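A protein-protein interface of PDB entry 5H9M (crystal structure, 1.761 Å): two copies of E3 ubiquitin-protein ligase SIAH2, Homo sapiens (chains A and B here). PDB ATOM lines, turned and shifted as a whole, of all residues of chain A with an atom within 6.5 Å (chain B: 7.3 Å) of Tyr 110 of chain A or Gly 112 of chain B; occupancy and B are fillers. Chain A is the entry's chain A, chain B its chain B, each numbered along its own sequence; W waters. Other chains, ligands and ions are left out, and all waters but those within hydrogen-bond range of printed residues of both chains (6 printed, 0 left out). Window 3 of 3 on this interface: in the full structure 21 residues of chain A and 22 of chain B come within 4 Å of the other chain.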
ATOM      1  N   GLN A 107      18.809  10.419  13.606  1.00  0.00           N
ATOM      2  CA  GLN A 107      19.452  11.731  13.605  1.00  0.00           C
ATOM      3  C   GLN A 107      18.417  12.763  13.188  1.00  0.00           C
ATOM      4  O   GLN A 107      17.618  12.528  12.280  1.00  0.00           O
ATOM      5  CB  GLN A 107      20.677  11.745  12.671  1.00  0.00           C
ATOM      6  CG  GLN A 107      21.439  13.060  12.652  1.00  0.00           C
ATOM      7  CD  GLN A 107      22.634  13.090  11.722  1.00  0.00           C
ATOM      8  OE1 GLN A 107      22.802  14.043  10.957  1.00  0.00           O
ATOM      9  NE2 GLN A 107      23.491  12.074  11.803  1.00  0.00           N
ATOM     10  N   GLU A 108      18.432  13.897  13.882  1.00  0.00           N
ATOM     11  CA  GLU A 108      17.633  15.047  13.511  1.00  0.00           C
ATOM     12  C   GLU A 108      18.533  15.967  12.687  1.00  0.00           C
ATOM     13  O   GLU A 108      19.134  16.919  13.209  1.00  0.00           O
ATOM     14  CB  GLU A 108      17.132  15.715  14.790  1.00  0.00           C
ATOM     15  CG  GLU A 108      15.890  16.533  14.632  1.00  0.00           C
ATOM     16  CD  GLU A 108      15.302  16.981  15.974  1.00  0.00           C
ATOM     17  OE1 GLU A 108      15.215  16.175  16.931  1.00  0.00           O
ATOM     18  OE2 GLU A 108      14.928  18.154  16.063  1.00  0.00           O
ATOM     19  N   LYS A 109      18.695  15.622  11.417  1.00  0.00           N
ATOM     20  CA  LYS A 109      19.578  16.358  10.511  1.00  0.00           C
ATOM     21  C   LYS A 109      18.933  17.703  10.170  1.00  0.00           C
ATOM     22  O   LYS A 109      19.549  18.768  10.314  1.00  0.00           O
ATOM     23  CB  LYS A 109      19.860  15.527   9.239  1.00  0.00           C
ATOM     24  CG  LYS A 109      20.844  16.163   8.285  1.00  0.00           C
ATOM     25  CD  LYS A 109      20.672  15.699   6.846  1.00  0.00           C
ATOM     26  CE  LYS A 109      20.985  14.249   6.691  1.00  0.00           C
ATOM     27  NZ  LYS A 109      20.956  13.874   5.240  1.00  0.00           N
ATOM     28  N   TYR A 110      17.687  17.635   9.717  1.00  0.00           N
ATOM     29  CA  TYR A 110      16.811  18.793   9.606  1.00  0.00           C
ATOM     30  C   TYR A 110      16.130  18.998  10.950  1.00  0.00           C
ATOM     31  O   TYR A 110      15.373  18.142  11.411  1.00  0.00           O
ATOM     32  CB  TYR A 110      15.768  18.597   8.484  1.00  0.00           C
ATOM     33  CG  TYR A 110      16.418  18.497   7.140  1.00  0.00           C
ATOM     34  CD1 TYR A 110      16.900  17.275   6.677  1.00  0.00           C
ATOM     35  CD2 TYR A 110      16.576  19.619   6.326  1.00  0.00           C
ATOM     36  CE1 TYR A 110      17.529  17.174   5.437  1.00  0.00           C
ATOM     37  CE2 TYR A 110      17.202  19.517   5.084  1.00  0.00           C
ATOM     38  CZ  TYR A 110      17.683  18.297   4.651  1.00  0.00           C
ATOM     39  OH  TYR A 110      18.312  18.155   3.433  1.00  0.00           O
ATOM     40  N   GLU A 111      16.362  20.154  11.577  1.00  0.00           N
ATOM     41  CA  GLU A 111      15.841  20.378  12.934  1.00  0.00           C
ATOM     42  C   GLU A 111      14.323  20.221  12.991  1.00  0.00           C
ATOM     43  O   GLU A 111      13.595  20.735  12.138  1.00  0.00           O
ATOM     44  CB  GLU A 111      16.269  21.756  13.467  1.00  0.00           C
ATOM     45  CG  GLU A 111      17.767  21.847  13.719  1.00  0.00           C
ATOM     46  CD  GLU A 111      18.617  22.113  12.474  1.00  0.00           C
ATOM     47  OE1 GLU A 111      18.052  22.318  11.368  1.00  0.00           O
ATOM     48  OE2 GLU A 111      19.860  22.103  12.584  1.00  0.00           O
ATOM     49  N   GLY A 112      13.874  19.452  13.977  1.00  0.00           N
ATOM     50  CA  GLY A 112      12.469  19.110  14.145  1.00  0.00           C
ATOM     51  C   GLY A 112      11.972  17.906  13.360  1.00  0.00           C
ATOM     52  O   GLY A 112      10.803  17.583  13.459  1.00  0.00           O
ATOM     53  N   HIS A 113      12.820  17.284  12.538  1.00  0.00           N
ATOM     54  CA  HIS A 113      12.429  16.091  11.773  1.00  0.00           C
ATOM     55  C   HIS A 113      13.389  14.942  12.074  1.00  0.00           C
ATOM     56  O   HIS A 113      14.476  14.883  11.533  1.00  0.00           O
ATOM     57  CB  HIS A 113      12.398  16.407  10.277  1.00  0.00           C
ATOM     58  CG  HIS A 113      11.874  15.289   9.438  1.00  0.00           C
ATOM     59  ND1 HIS A 113      12.141  15.193   8.092  1.00  0.00           N
ATOM     60  CD2 HIS A 113      11.140  14.200   9.751  1.00  0.00           C
ATOM     61  CE1 HIS A 113      11.572  14.111   7.600  1.00  0.00           C
ATOM     62  NE2 HIS A 113      10.967  13.483   8.591  1.00  0.00           N
ATOM     63  N   GLN A 114      12.976  14.023  12.946  1.00  0.00           N
ATOM     64  CA  GLN A 114      13.813  12.881  13.277  1.00  0.00           C
ATOM     65  C   GLN A 114      13.746  11.903  12.131  1.00  0.00           C
ATOM     66  O   GLN A 114      12.673  11.477  11.742  1.00  0.00           O
ATOM     67  CB  GLN A 114      13.321  12.173  14.543  1.00  0.00           C
ATOM     68  CG  GLN A 114      13.551  12.952  15.816  1.00  0.00           C
ATOM     69  CD  GLN A 114      13.332  12.059  17.029  1.00  0.00           C
ATOM     70  OE1 GLN A 114      12.262  11.468  17.176  1.00  0.00           O
ATOM     71  NE2 GLN A 114      14.352  11.908  17.860  1.00  0.00           N
ATOM     72  N   GLN A 115      14.903  11.536  11.617  1.00  0.00           N
ATOM     73  CA  GLN A 115      14.978  10.586  10.519  1.00  0.00           C
ATOM     74  C   GLN A 115      15.839   9.417  10.938  1.00  0.00           C
ATOM     75  O   GLN A 115      16.647   9.519  11.882  1.00  0.00           O
ATOM     76  CB  GLN A 115      15.555  11.271   9.276  1.00  0.00           C
ATOM     77  CG  GLN A 115      14.532  12.108   8.528  1.00  0.00           C
ATOM     78  CD  GLN A 115      15.118  12.704   7.272  1.00  0.00           C
ATOM     79  OE1 GLN A 115      16.058  13.482   7.340  1.00  0.00           O
ATOM     80  NE2 GLN A 115      14.578  12.324   6.107  1.00  0.00           N
ATOM     81  N   MET A 163      24.992  12.229   5.496  1.00  0.00           N
ATOM     82  CA  MET A 163      24.932  13.610   5.026  1.00  0.00           C
ATOM     83  C   MET A 163      24.370  13.711   3.614  1.00  0.00           C
ATOM     84  O   MET A 163      23.609  14.622   3.330  1.00  0.00           O
ATOM     85  CB  MET A 163      26.301  14.305   5.107  1.00  0.00           C
ATOM     86  CG  MET A 163      26.203  15.827   4.959  1.00  0.00           C
ATOM     87  N   SER A 165      22.317  11.392   2.206  1.00  0.00           N
ATOM     88  CA  SER A 165      21.173  10.478   2.090  1.00  0.00           C
ATOM     89  C   SER A 165      21.420   9.292   1.140  1.00  0.00           C
ATOM     90  O   SER A 165      20.496   8.844   0.443  1.00  0.00           O
ATOM     91  CB  SER A 165      19.914  11.245   1.667  1.00  0.00           C
ATOM     92  OG  SER A 165      19.622  12.262   2.591  1.00  0.00           O
ATOM     93  N   GLU B 108       7.477  21.012   1.830  1.00  0.00           N
ATOM     94  CA  GLU B 108       8.010  21.006   3.187  1.00  0.00           C
ATOM     95  C   GLU B 108       6.922  20.514   4.106  1.00  0.00           C
ATOM     96  O   GLU B 108       6.213  21.305   4.751  1.00  0.00           O
ATOM     97  CB  GLU B 108       8.490  22.395   3.623  1.00  0.00           C
ATOM     98  CG  GLU B 108       9.674  22.910   2.837  1.00  0.00           C
ATOM     99  CD  GLU B 108      10.033  24.348   3.189  1.00  0.00           C
ATOM    100  OE1 GLU B 108       9.823  24.754   4.350  1.00  0.00           O
ATOM    101  OE2 GLU B 108      10.534  25.058   2.294  1.00  0.00           O
ATOM    102  N   LYS B 109       6.783  19.198   4.165  1.00  0.00           N
ATOM    103  CA  LYS B 109       5.844  18.583   5.089  1.00  0.00           C
ATOM    104  C   LYS B 109       6.306  18.876   6.503  1.00  0.00           C
ATOM    105  O   LYS B 109       5.520  19.302   7.317  1.00  0.00           O
ATOM    106  CB  LYS B 109       5.721  17.089   4.865  1.00  0.00           C
ATOM    107  CG  LYS B 109       4.851  16.374   5.891  1.00  0.00           C
ATOM    108  CD  LYS B 109       4.597  14.962   5.408  1.00  0.00           C
ATOM    109  CE  LYS B 109       4.322  13.998   6.527  1.00  0.00           C
ATOM    110  NZ  LYS B 109       4.431  12.628   5.983  1.00  0.00           N
ATOM    111  N   TYR B 110       7.586  18.634   6.770  1.00  0.00           N
ATOM    112  CA  TYR B 110       8.236  19.116   7.982  1.00  0.00           C
ATOM    113  C   TYR B 110       8.886  20.452   7.669  1.00  0.00           C
ATOM    114  O   TYR B 110       9.546  20.615   6.638  1.00  0.00           O
ATOM    115  CB  TYR B 110       9.281  18.117   8.477  1.00  0.00           C
ATOM    116  CG  TYR B 110       8.691  16.794   8.889  1.00  0.00           C
ATOM    117  CD1 TYR B 110       8.449  15.808   7.944  1.00  0.00           C
ATOM    118  CD2 TYR B 110       8.374  16.514  10.226  1.00  0.00           C
ATOM    119  CE1 TYR B 110       7.892  14.586   8.290  1.00  0.00           C
ATOM    120  CE2 TYR B 110       7.819  15.278  10.581  1.00  0.00           C
ATOM    121  CZ  TYR B 110       7.589  14.320   9.600  1.00  0.00           C
ATOM    122  OH  TYR B 110       7.053  13.067   9.876  1.00  0.00           O
ATOM    123  N   GLU B 111       8.692  21.404   8.569  1.00  0.00           N
ATOM    124  CA  GLU B 111       9.165  22.783   8.403  1.00  0.00           C
ATOM    125  C   GLU B 111      10.648  22.856   8.016  1.00  0.00           C
ATOM    126  O   GLU B 111      11.501  22.320   8.699  1.00  0.00           O
ATOM    127  CB  GLU B 111       8.937  23.561   9.721  1.00  0.00           C
ATOM    128  CG  GLU B 111       9.293  25.042   9.674  1.00  0.00           C
ATOM    129  CD  GLU B 111       8.378  25.831   8.755  1.00  0.00           C
ATOM    130  OE1 GLU B 111       7.147  25.827   8.991  1.00  0.00           O
ATOM    131  OE2 GLU B 111       8.887  26.463   7.802  1.00  0.00           O
ATOM    132  N   GLY B 112      10.933  23.507   6.893  1.00  0.00           N
ATOM    133  CA  GLY B 112      12.286  23.671   6.429  1.00  0.00           C
ATOM    134  C   GLY B 112      12.935  22.428   5.843  1.00  0.00           C
ATOM    135  O   GLY B 112      14.150  22.423   5.629  1.00  0.00           O
ATOM    136  N   HIS B 113      12.154  21.385   5.568  1.00  0.00           N
ATOM    137  CA  HIS B 113      12.722  20.197   4.936  1.00  0.00           C
ATOM    138  C   HIS B 113      11.904  19.857   3.713  1.00  0.00           C
ATOM    139  O   HIS B 113      10.835  19.251   3.816  1.00  0.00           O
ATOM    140  CB  HIS B 113      12.799  19.005   5.891  1.00  0.00           C
ATOM    141  CG  HIS B 113      13.519  17.826   5.294  1.00  0.00           C
ATOM    142  ND1 HIS B 113      13.516  16.586   5.872  1.00  0.00           N
ATOM    143  CD2 HIS B 113      14.251  17.706   4.165  1.00  0.00           C
ATOM    144  CE1 HIS B 113      14.243  15.754   5.154  1.00  0.00           C
ATOM    145  NE2 HIS B 113      14.682  16.403   4.094  1.00  0.00           N
ATOM    146  N   GLN B 114      12.412  20.268   2.561  1.00  0.00           N
ATOM    147  CA  GLN B 114      11.747  19.983   1.289  1.00  0.00           C
ATOM    148  C   GLN B 114      11.943  18.502   0.976  1.00  0.00           C
ATOM    149  O   GLN B 114      13.060  18.040   0.925  1.00  0.00           O
ATOM    150  CB  GLN B 114      12.330  20.859   0.181  1.00  0.00           C
ATOM    151  CG  GLN B 114      12.080  22.350   0.438  1.00  0.00           C
ATOM    152  CD  GLN B 114      12.658  23.305  -0.606  1.00  0.00           C
ATOM    153  OE1 GLN B 114      11.929  23.799  -1.478  1.00  0.00           O
ATOM    154  NE2 GLN B 114      13.959  23.601  -0.501  1.00  0.00           N
ATOM    155  N   GLN B 115      10.859  17.763   0.791  1.00  0.00           N
ATOM    156  CA  GLN B 115      10.961  16.362   0.395  1.00  0.00           C
ATOM    157  C   GLN B 115      10.050  16.088  -0.793  1.00  0.00           C
ATOM    158  O   GLN B 115       9.174  16.892  -1.100  1.00  0.00           O
ATOM    159  CB  GLN B 115      10.568  15.426   1.537  1.00  0.00           C
ATOM    160  CG  GLN B 115      11.543  15.461   2.703  1.00  0.00           C
ATOM    161  CD  GLN B 115      11.200  14.451   3.771  1.00  0.00           C
ATOM    162  OE1 GLN B 115      10.156  14.545   4.430  1.00  0.00           O
ATOM    163  NE2 GLN B 115      12.073  13.437   3.924  1.00  0.00           N
ATOM    164  N   ASP B 171      14.249  12.323   0.274  1.00  0.00           N
ATOM    165  CA  ASP B 171      14.967  13.586   0.359  1.00  0.00           C
ATOM    166  C   ASP B 171      15.322  14.138  -1.026  1.00  0.00           C
ATOM    167  O   ASP B 171      15.498  13.386  -2.029  1.00  0.00           O
ATOM    168  CB  ASP B 171      16.297  13.411   1.125  1.00  0.00           C
ATOM    169  CG  ASP B 171      16.105  12.998   2.591  1.00  0.00           C
ATOM    170  OD1 ASP B 171      15.054  13.303   3.193  1.00  0.00           O
ATOM    171  OD2 ASP B 171      17.039  12.382   3.145  1.00  0.00           O
ATOM    172  N   THR B 172      15.445  15.456  -1.067  1.00  0.00           N
ATOM    173  CA  THR B 172      15.920  16.171  -2.231  1.00  0.00           C
ATOM    174  C   THR B 172      17.265  15.620  -2.730  1.00  0.00           C
ATOM    175  O   THR B 172      17.459  15.450  -3.932  1.00  0.00           O
ATOM    176  CB  THR B 172      16.019  17.658  -1.881  1.00  0.00           C
ATOM    177  OG1 THR B 172      14.685  18.181  -1.738  1.00  0.00           O
ATOM    178  CG2 THR B 172      16.788  18.406  -2.938  1.00  0.00           C
ATOM    179  N   ALA B 173      18.156  15.289  -1.796  1.00  0.00           N
ATOM    180  CA  ALA B 173      19.447  14.666  -2.114  1.00  0.00           C
ATOM    181  C   ALA B 173      19.260  13.342  -2.854  1.00  0.00           C
ATOM    182  O   ALA B 173      19.999  13.039  -3.765  1.00  0.00           O
ATOM    183  CB  ALA B 173      20.254  14.426  -0.853  1.00  0.00           C
HETATM  184  O   HOH W   1      15.800  16.756   1.594  1.00  0.00           O
HETATM  185  O   HOH W   2      11.323  20.207  10.627  1.00  0.00           O
HETATM  186  O   HOH W   3      18.401  16.217   1.091  1.00  0.00           O
HETATM  187  O   HOH W   4      18.091  13.659   5.297  1.00  0.00           O
HETATM  188  O   HOH W   5      11.936  10.807   5.786  1.00  0.00           O
HETATM  189  O   HOH W   6       9.412  11.716  11.572  1.00  0.00           O
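Tyr 110 of chain A touches His 113 of chain B, and with the chains exchanged His 113 of chain A touches Tyr 110 of chain B. His 113 of chain B touches its own counterpart, His 113 of chain A. His 113 of chain A touches Gln 115 of chain B, and with the chains exchanged Gln 115 of chain A touches His 113 of chain B. Gln 115 of chain A touches its own counterpart, Gln 115 of chain B. Of the 9 pairs that touch across the chains among the printed residues, 6 have their exchanged pair printed and touching as well.
Among the printed residues, merely in contact across the chains: Tyr 110 of chain A with His 113 of chain B (3.2 Å), His 113 of chain A with Tyr 110 of chain B (3.3 Å), His 113 of chain A with Gln 115 of chain B (3.5 Å), Gln 115 of chain A with Gln 115 of chain B (3.5 Å), Gln 115 of chain A with His 113 of chain B (3.6 Å) and Tyr 110 of chain A with Gly 112 of chain B (3.8 Å).
Water W4 lies within hydrogen-bond range of OD2 of Asp 171 of chain B, NZ of Lys 109 of chain A, OE1 of Gln 115 of chain A and OG of Ser 165 of chain A. Water W1 lies within hydrogen-bond range of a ring nitrogen (NE2) of His 113 of chain B (2.8 Å), the backbone NH of Thr 172 of chain B (3.0 Å), the backbone carbonyl oxygen of Gln 114 of chain B (3.1 Å) and the side-chain hydroxyl of Tyr 110 of chain A (3.4 Å). Water W2 bridges the backbone carbonyl oxygen of Glu 111 of chain A (2.8 Å) and the backbone carbonyl oxygen of Glu 111 of chain B (2.9 Å). Water W3 bridges the side-chain hydroxyl (OH) of Tyr 110 of chain A and the backbone NH (N) of Ala 173 of chain B. Water W5 lies within hydrogen-bond range of the side-chain amide nitrogen (NE2) of Gln 115 of chain A (3.1 Å) and the side-chain amide nitrogen (NE2) of Gln 115 of chain B (3.2 Å). Water W6 lies within hydrogen-bond range of OH of Tyr 110 of chain B (3.2 Å) and O of Gln 114 of chain A (3.3 Å).
Hydrophobic or aromatic side chains of chain B within 4 Å of the printed part of chain A: Tyr 110 and His 113. Printed residues of chain A that touch a printed residue of chain B: Tyr 110, His 113, Gln 115 and Ser 165. Among the printed residues, no Asp or Glu carboxylate lies within 4 Å of a Lys or Arg side-chain nitrogen of the other chain.
Tyr 110 of chain A touches two residues of chain B. Printed residues of chain B within 4 Å of His 113 of chain A: Tyr 110, His 113 and Gln 115. Of the printed residues of chain B, Ser 165 of chain A touches Asp 171. Of the printed residues of chain A, Tyr 110 of chain B touches His 113 (3.3 Å). Gly 112 of chain B touches just one residue of chain A: Tyr 110. Of the printed residues of chain A, His 113 of chain B touches Tyr 110 (3.2 Å), His 113 (3.0 Å) and Gln 115 (3.6 Å). Of the printed residues of chain A, Asp 171 of chain B touches Gln 115 (3.1 Å) and Ser 165 (2.6 Å).
The side-chain hydroxyl (OG) of Ser 165 of chain A lies within hydrogen-bond range of the side-chain carboxylate (OD2) of Asp 171 of chain B, 2.6 Å away. A ring nitrogen (ND1) of His 113 of chain B is in hydrogen-bond range of a ring nitrogen (ND1) of His 113 of chain A (3.0 Å). NE2 of Gln 115 of chain A sits at hydrogen-bond distance from OD1 of Asp 171 of chain B (3.1 Å).
The backbone NH (N) of Gln 107 of chain A lies within hydrogen-bond range of the backbone carbonyl oxygen (O) of Gln 115 of chain A, at 2.9 Å. The side-chain carboxylate (OE1) of Glu 108 of chain B sits at hydrogen-bond distance from the backbone NH (N) of Gly 112 of chain B, at 3.0 Å. OD1 of Asp 171 of chain B lies within hydrogen-bond range of NE2 of Gln 115 of chain B (3.1 Å). A ring nitrogen (NE2) of His 113 of chain B lies close to the side-chain carboxylate (OD1) of Asp 171 of chain B (3.2 Å). OG of Ser 165 of chain A lies within hydrogen-bond range of NZ of Lys 109 of chain A (3.4 Å).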
